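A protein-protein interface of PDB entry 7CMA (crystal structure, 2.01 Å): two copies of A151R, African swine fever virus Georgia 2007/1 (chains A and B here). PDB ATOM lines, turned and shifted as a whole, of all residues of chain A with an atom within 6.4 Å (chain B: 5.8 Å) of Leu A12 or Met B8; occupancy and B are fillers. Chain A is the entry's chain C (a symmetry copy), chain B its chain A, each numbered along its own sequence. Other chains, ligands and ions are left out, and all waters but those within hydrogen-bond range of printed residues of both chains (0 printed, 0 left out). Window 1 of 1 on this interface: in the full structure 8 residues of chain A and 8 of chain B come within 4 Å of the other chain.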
ATOM      1  N   VAL A   7      21.974 -18.957 -22.885  1.00  0.00           N
ATOM      2  CA  VAL A   7      21.551 -18.184 -21.681  1.00  0.00           C
ATOM      3  C   VAL A   7      22.785 -17.891 -20.821  1.00  0.00           C
ATOM      4  O   VAL A   7      22.990 -16.717 -20.466  1.00  0.00           O
ATOM      5  CB  VAL A   7      20.468 -18.933 -20.883  1.00  0.00           C
ATOM      6  CG1 VAL A   7      20.333 -18.400 -19.463  1.00  0.00           C
ATOM      7  CG2 VAL A   7      19.125 -18.896 -21.597  1.00  0.00           C
ATOM      8  N   MET A   8      23.622 -18.900 -20.579  1.00  0.00           N
ATOM      9  CA  MET A   8      24.856 -18.763 -19.764  1.00  0.00           C
ATOM     10  C   MET A   8      25.769 -17.716 -20.404  1.00  0.00           C
ATOM     11  O   MET A   8      26.317 -16.893 -19.665  1.00  0.00           O
ATOM     12  CB  MET A   8      25.601 -20.097 -19.647  1.00  0.00           C
ATOM     13  CG  MET A   8      25.379 -20.787 -18.320  1.00  0.00           C
ATOM     14  SD  MET A   8      26.293 -22.348 -18.183  1.00  0.00           S
ATOM     15  CE  MET A   8      25.129 -23.453 -18.969  1.00  0.00           C
ATOM     16  N   MET A   9      25.868 -17.712 -21.736  1.00  0.00           N
ATOM     17  CA  MET A   9      26.723 -16.771 -22.501  1.00  0.00           C
ATOM     18  C   MET A   9      26.196 -15.342 -22.326  1.00  0.00           C
ATOM     19  O   MET A   9      27.030 -14.434 -22.144  1.00  0.00           O
ATOM     20  CB  MET A   9      26.756 -17.132 -23.990  1.00  0.00           C
ATOM     21  CG  MET A   9      27.778 -18.214 -24.321  1.00  0.00           C
ATOM     22  SD  MET A   9      27.545 -18.914 -25.982  1.00  0.00           S
ATOM     23  CE  MET A   9      27.956 -17.492 -26.992  1.00  0.00           C
ATOM     24  N   ALA A  10      24.869 -15.159 -22.342  1.00  0.00           N
ATOM     25  CA  ALA A  10      24.225 -13.829 -22.191  1.00  0.00           C
ATOM     26  C   ALA A  10      24.417 -13.307 -20.757  1.00  0.00           C
ATOM     27  O   ALA A  10      24.637 -12.097 -20.599  1.00  0.00           O
ATOM     28  CB  ALA A  10      22.762 -13.912 -22.555  1.00  0.00           C
ATOM     29  N   LEU A  11      24.280 -14.174 -19.751  1.00  0.00           N
ATOM     30  CA  LEU A  11      24.443 -13.780 -18.323  1.00  0.00           C
ATOM     31  C   LEU A  11      25.918 -13.459 -18.054  1.00  0.00           C
ATOM     32  O   LEU A  11      26.185 -12.541 -17.259  1.00  0.00           O
ATOM     33  CB  LEU A  11      23.937 -14.903 -17.416  1.00  0.00           C
ATOM     34  CG  LEU A  11      22.429 -15.150 -17.466  1.00  0.00           C
ATOM     35  CD1 LEU A  11      22.002 -16.123 -16.376  1.00  0.00           C
ATOM     36  CD2 LEU A  11      21.658 -13.842 -17.347  1.00  0.00           C
ATOM     37  N   LEU A  12      26.833 -14.145 -18.742  1.00  0.00           N
ATOM     38  CA  LEU A  12      28.291 -13.913 -18.587  1.00  0.00           C
ATOM     39  C   LEU A  12      28.663 -12.571 -19.232  1.00  0.00           C
ATOM     40  O   LEU A  12      29.399 -11.799 -18.592  1.00  0.00           O
ATOM     41  CB  LEU A  12      29.072 -15.064 -19.222  1.00  0.00           C
ATOM     42  CG  LEU A  12      30.589 -14.901 -19.197  1.00  0.00           C
ATOM     43  CD1 LEU A  12      31.106 -14.876 -17.765  1.00  0.00           C
ATOM     44  CD2 LEU A  12      31.272 -16.001 -19.996  1.00  0.00           C
ATOM     45  N   HIS A  13      28.149 -12.294 -20.434  1.00  0.00           N
ATOM     46  CA  HIS A  13      28.319 -10.981 -21.117  1.00  0.00           C
ATOM     47  C   HIS A  13      27.785  -9.863 -20.217  1.00  0.00           C
ATOM     48  O   HIS A  13      28.531  -8.900 -19.986  1.00  0.00           O
ATOM     49  CB  HIS A  13      27.643 -10.984 -22.494  1.00  0.00           C
ATOM     50  CG  HIS A  13      27.518  -9.625 -23.099  1.00  0.00           C
ATOM     51  ND1 HIS A  13      28.582  -8.989 -23.713  1.00  0.00           N
ATOM     52  CD2 HIS A  13      26.478  -8.762 -23.150  1.00  0.00           C
ATOM     53  CE1 HIS A  13      28.189  -7.814 -24.159  1.00  0.00           C
ATOM     54  NE2 HIS A  13      26.905  -7.643 -23.813  1.00  0.00           N
ATOM     55  N   LYS A  14      26.601 -10.058 -19.629  1.00  0.00           N
ATOM     56  CA  LYS A  14      25.996  -9.110 -18.654  1.00  0.00           C
ATOM     57  C   LYS A  14      26.997  -8.837 -17.522  1.00  0.00           C
ATOM     58  O   LYS A  14      27.290  -7.654 -17.260  1.00  0.00           O
ATOM     59  CB  LYS A  14      24.683  -9.672 -18.101  1.00  0.00           C
ATOM     60  CG  LYS A  14      24.164  -8.990 -16.843  1.00  0.00           C
ATOM     61  CD  LYS A  14      22.811  -9.492 -16.397  1.00  0.00           C
ATOM     62  CE  LYS A  14      22.076  -8.500 -15.520  1.00  0.00           C
ATOM     63  NZ  LYS A  14      20.682  -8.931 -15.261  1.00  0.00           N
ATOM     64  N   GLU A  15      27.445  -9.886 -16.828  1.00  0.00           N
ATOM     65  CA  GLU A  15      28.329  -9.759 -15.642  1.00  0.00           C
ATOM     66  C   GLU A  15      29.602  -9.002 -16.043  1.00  0.00           C
ATOM     67  O   GLU A  15      30.036  -8.135 -15.270  1.00  0.00           O
ATOM     68  CB  GLU A  15      28.649 -11.133 -15.054  1.00  0.00           C
ATOM     69  CG  GLU A  15      28.466 -11.192 -13.546  1.00  0.00           C
ATOM     70  CD  GLU A  15      27.170 -10.577 -13.036  1.00  0.00           C
ATOM     71  OE1 GLU A  15      26.119 -10.770 -13.689  1.00  0.00           O
ATOM     72  OE2 GLU A  15      27.222  -9.875 -12.011  1.00  0.00           O
ATOM     73  N   LYS A  16      30.139  -9.283 -17.234  1.00  0.00           N
ATOM     74  CA  LYS A  16      31.413  -8.678 -17.700  1.00  0.00           C
ATOM     75  C   LYS A  16      31.166  -7.204 -18.053  1.00  0.00           C
ATOM     76  O   LYS A  16      31.972  -6.373 -17.647  1.00  0.00           O
ATOM     77  CB  LYS A  16      31.983  -9.462 -18.885  1.00  0.00           C
ATOM     78  CG  LYS A  16      32.644 -10.789 -18.525  1.00  0.00           C
ATOM     79  CD  LYS A  16      33.705 -11.240 -19.515  1.00  0.00           C
ATOM     80  CE  LYS A  16      33.284 -12.433 -20.347  1.00  0.00           C
ATOM     81  NZ  LYS A  16      32.251 -12.073 -21.350  1.00  0.00           N
ATOM     82  N   LEU A  17      30.030  -6.891 -18.678  1.00  0.00           N
ATOM     83  CA  LEU A  17      29.749  -5.517 -19.178  1.00  0.00           C
ATOM     84  C   LEU A  17      29.385  -4.619 -17.991  1.00  0.00           C
ATOM     85  O   LEU A  17      29.973  -3.539 -17.890  1.00  0.00           O
ATOM     86  CB  LEU A  17      28.626  -5.558 -20.219  1.00  0.00           C
ATOM     87  CG  LEU A  17      28.270  -4.211 -20.853  1.00  0.00           C
ATOM     88  CD1 LEU A  17      29.518  -3.469 -21.314  1.00  0.00           C
ATOM     89  CD2 LEU A  17      27.302  -4.396 -22.014  1.00  0.00           C
ATOM     90  N   LYS B   3      35.377 -12.755  -9.094  1.00  0.00           N
ATOM     91  CA  LYS B   3      35.381 -14.213  -8.797  1.00  0.00           C
ATOM     92  C   LYS B   3      34.139 -14.856  -9.423  1.00  0.00           C
ATOM     93  O   LYS B   3      34.261 -15.973  -9.961  1.00  0.00           O
ATOM     94  CB  LYS B   3      35.424 -14.453  -7.285  1.00  0.00           C
ATOM     95  CG  LYS B   3      35.812 -15.866  -6.866  1.00  0.00           C
ATOM     96  CD  LYS B   3      35.475 -16.192  -5.423  1.00  0.00           C
ATOM     97  CE  LYS B   3      36.002 -15.170  -4.437  1.00  0.00           C
ATOM     98  NZ  LYS B   3      37.469 -15.286  -4.254  1.00  0.00           N
ATOM     99  N   LYS B   4      32.996 -14.164  -9.364  1.00  0.00           N
ATOM    100  CA  LYS B   4      31.706 -14.665  -9.904  1.00  0.00           C
ATOM    101  C   LYS B   4      31.842 -14.869 -11.417  1.00  0.00           C
ATOM    102  O   LYS B   4      31.271 -15.853 -11.936  1.00  0.00           O
ATOM    103  CB  LYS B   4      30.569 -13.695  -9.574  1.00  0.00           C
ATOM    104  CG  LYS B   4      29.214 -14.351  -9.352  1.00  0.00           C
ATOM    105  CD  LYS B   4      28.045 -13.417  -9.572  1.00  0.00           C
ATOM    106  CE  LYS B   4      26.788 -14.136 -10.010  1.00  0.00           C
ATOM    107  NZ  LYS B   4      25.907 -13.252 -10.810  1.00  0.00           N
ATOM    108  N   ILE B   5      32.629 -14.021 -12.080  1.00  0.00           N
ATOM    109  CA  ILE B   5      32.864 -14.105 -13.551  1.00  0.00           C
ATOM    110  C   ILE B   5      33.800 -15.291 -13.835  1.00  0.00           C
ATOM    111  O   ILE B   5      33.551 -16.009 -14.813  1.00  0.00           O
ATOM    112  CB  ILE B   5      33.415 -12.774 -14.104  1.00  0.00           C
ATOM    113  CG1 ILE B   5      32.366 -11.661 -14.030  1.00  0.00           C
ATOM    114  CG2 ILE B   5      33.950 -12.952 -15.518  1.00  0.00           C
ATOM    115  CD1 ILE B   5      32.845 -10.319 -14.548  1.00  0.00           C
ATOM    116  N   ILE B   6      34.761 -15.558 -12.944  1.00  0.00           N
ATOM    117  CA  ILE B   6      35.723 -16.689 -13.131  1.00  0.00           C
ATOM    118  C   ILE B   6      34.965 -18.010 -12.937  1.00  0.00           C
ATOM    119  O   ILE B   6      35.128 -18.903 -13.787  1.00  0.00           O
ATOM    120  CB  ILE B   6      36.940 -16.569 -12.187  1.00  0.00           C
ATOM    121  CG1 ILE B   6      38.147 -15.938 -12.889  1.00  0.00           C
ATOM    122  CG2 ILE B   6      37.294 -17.925 -11.589  1.00  0.00           C
ATOM    123  CD1 ILE B   6      38.006 -14.458 -13.162  1.00  0.00           C
ATOM    124  N   VAL B   7      34.019 -18.036 -11.990  1.00  0.00           N
ATOM    125  CA  VAL B   7      33.137 -19.214 -11.728  1.00  0.00           C
ATOM    126  C   VAL B   7      32.203 -19.408 -12.925  1.00  0.00           C
ATOM    127  O   VAL B   7      32.142 -20.538 -13.453  1.00  0.00           O
ATOM    128  CB  VAL B   7      32.348 -19.046 -10.415  1.00  0.00           C
ATOM    129  CG1 VAL B   7      31.188 -20.027 -10.315  1.00  0.00           C
ATOM    130  CG2 VAL B   7      33.256 -19.171  -9.201  1.00  0.00           C
ATOM    131  N   MET B   8      31.579 -18.329 -13.400  1.00  0.00           N
ATOM    132  CA  MET B   8      30.639 -18.387 -14.546  1.00  0.00           C
ATOM    133  C   MET B   8      31.378 -18.923 -15.778  1.00  0.00           C
ATOM    134  O   MET B   8      30.794 -19.746 -16.494  1.00  0.00           O
ATOM    135  CB  MET B   8      30.051 -17.009 -14.857  1.00  0.00           C
ATOM    136  CG  MET B   8      28.622 -16.851 -14.386  1.00  0.00           C
ATOM    137  SD  MET B   8      27.969 -15.196 -14.719  1.00  0.00           S
ATOM    138  CE  MET B   8      28.671 -14.314 -13.332  1.00  0.00           C
ATOM    139  N   MET B   9      32.624 -18.493 -15.990  1.00  0.00           N
ATOM    140  CA  MET B   9      33.451 -18.909 -17.149  1.00  0.00           C
ATOM    141  C   MET B   9      33.739 -20.412 -17.051  1.00  0.00           C
ATOM    142  O   MET B   9      33.694 -21.082 -18.096  1.00  0.00           O
ATOM    143  CB  MET B   9      34.771 -18.134 -17.205  1.00  0.00           C
ATOM    144  CG  MET B   9      34.644 -16.762 -17.862  1.00  0.00           C
ATOM    145  SD  MET B   9      36.079 -15.697 -17.519  1.00  0.00           S
ATOM    146  CE  MET B   9      37.345 -16.556 -18.451  1.00  0.00           C
ATOM    147  N   ALA B  10      34.000 -20.921 -15.839  1.00  0.00           N
ATOM    148  CA  ALA B  10      34.323 -22.354 -15.612  1.00  0.00           C
ATOM    149  C   ALA B  10      33.075 -23.217 -15.849  1.00  0.00           C
ATOM    150  O   ALA B  10      33.216 -24.311 -16.428  1.00  0.00           O
ATOM    151  CB  ALA B  10      34.874 -22.553 -14.222  1.00  0.00           C
ATOM    152  N   LEU B  11      31.904 -22.757 -15.397  1.00  0.00           N
ATOM    153  CA  LEU B  11      30.627 -23.509 -15.540  1.00  0.00           C
ATOM    154  C   LEU B  11      30.193 -23.485 -17.009  1.00  0.00           C
ATOM    155  O   LEU B  11      29.610 -24.480 -17.468  1.00  0.00           O
ATOM    156  CB  LEU B  11      29.561 -22.895 -14.629  1.00  0.00           C
ATOM    157  CG  LEU B  11      29.804 -23.068 -13.129  1.00  0.00           C
ATOM    158  CD1 LEU B  11      28.593 -22.614 -12.327  1.00  0.00           C
ATOM    159  CD2 LEU B  11      30.157 -24.510 -12.795  1.00  0.00           C
ATOM    160  N   LEU B  12      30.499 -22.404 -17.727  1.00  0.00           N
ATOM    161  CA  LEU B  12      30.208 -22.285 -19.178  1.00  0.00           C
ATOM    162  C   LEU B  12      31.122 -23.239 -19.963  1.00  0.00           C
ATOM    163  O   LEU B  12      30.604 -23.954 -20.837  1.00  0.00           O
ATOM    164  CB  LEU B  12      30.399 -20.837 -19.630  1.00  0.00           C
ATOM    165  CG  LEU B  12      30.218 -20.607 -21.129  1.00  0.00           C
ATOM    166  CD1 LEU B  12      28.798 -20.954 -21.559  1.00  0.00           C
ATOM    167  CD2 LEU B  12      30.561 -19.175 -21.510  1.00  0.00           C
ATOM    168  N   HIS B  13      32.427 -23.234 -19.672  1.00  0.00           N
ATOM    169  CA  HIS B  13      33.393 -24.199 -20.269  1.00  0.00           C
ATOM    170  C   HIS B  13      32.901 -25.631 -20.039  1.00  0.00           C
ATOM    171  O   HIS B  13      32.818 -26.386 -21.024  1.00  0.00           O
ATOM    172  CB  HIS B  13      34.806 -23.982 -19.709  1.00  0.00           C
ATOM    173  CG  HIS B  13      35.760 -25.082 -20.043  1.00  0.00           C
ATOM    174  ND1 HIS B  13      36.381 -25.172 -21.277  1.00  0.00           N
ATOM    175  CD2 HIS B  13      36.189 -26.144 -19.323  1.00  0.00           C
ATOM    176  CE1 HIS B  13      37.177 -26.221 -21.288  1.00  0.00           C
ATOM    177  NE2 HIS B  13      37.064 -26.845 -20.108  1.00  0.00           N
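Of the printed residues of chain B, Met A8 touches Leu B12 (3.8 Å). Of the printed residues of chain B, Leu A12 touches Ile B5, Met B8 and Leu B12. Printed residues of chain A within 4 Å of Lys B4: Glu A15 (3.7 Å). Val B7 touches none of the printed residues of chain A. Met B8 touches just these residues of chain A: Leu A12 and Glu A15. The nearest residue of chain A that does not touch Met B8 is Leu A11 (4.1 Å). The nearest printed residue of chain B that does not touch Glu A15 is Ile B6 (7.7 Å).
Hydrophobic or aromatic side chains of chain A within 4 Å of the printed part of chain B: Met A8 and Leu A12. Of the 11 printed residues of chain B, 4 touch a printed residue of chain A. Hydrophobic or aromatic side chains of chain B that line the printed part of chain A: Ile B5, Met B8 and Leu B12. Along chain B the printed residues that touch a printed residue of chain A span positions 4 to 12. Among the printed residues, 8 pairs touch across the chains. Among the printed residues, Asp or Glu carboxylates within 4 Å of a Lys or Arg side-chain nitrogen of the other chain: Glu A15 with Lys B4.
Met A8 touches Leu B12, and with the chains exchanged Leu A12 touches Met B8. Leu B12 touches its own counterpart, Leu A12.
The side-chain carboxylate (OE1) of Glu A15 is in salt-bridge range of the side-chain amino group (NZ) of Lys B4, 3.8 Å away.
Among the printed residues, pairs that only touch across the chains: Glu A15 with Met B8 (3.1 Å), Leu A12 with Leu B12 (3.6 Å), Glu A15 with Ile B5 (3.6 Å), Leu A12 with Met B8 (3.8 Å), Met A8 with Leu B12 (3.8 Å), Lys A16 with Ile B5 (3.8 Å) and Leu A12 with Ile B5 (3.997 Å).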
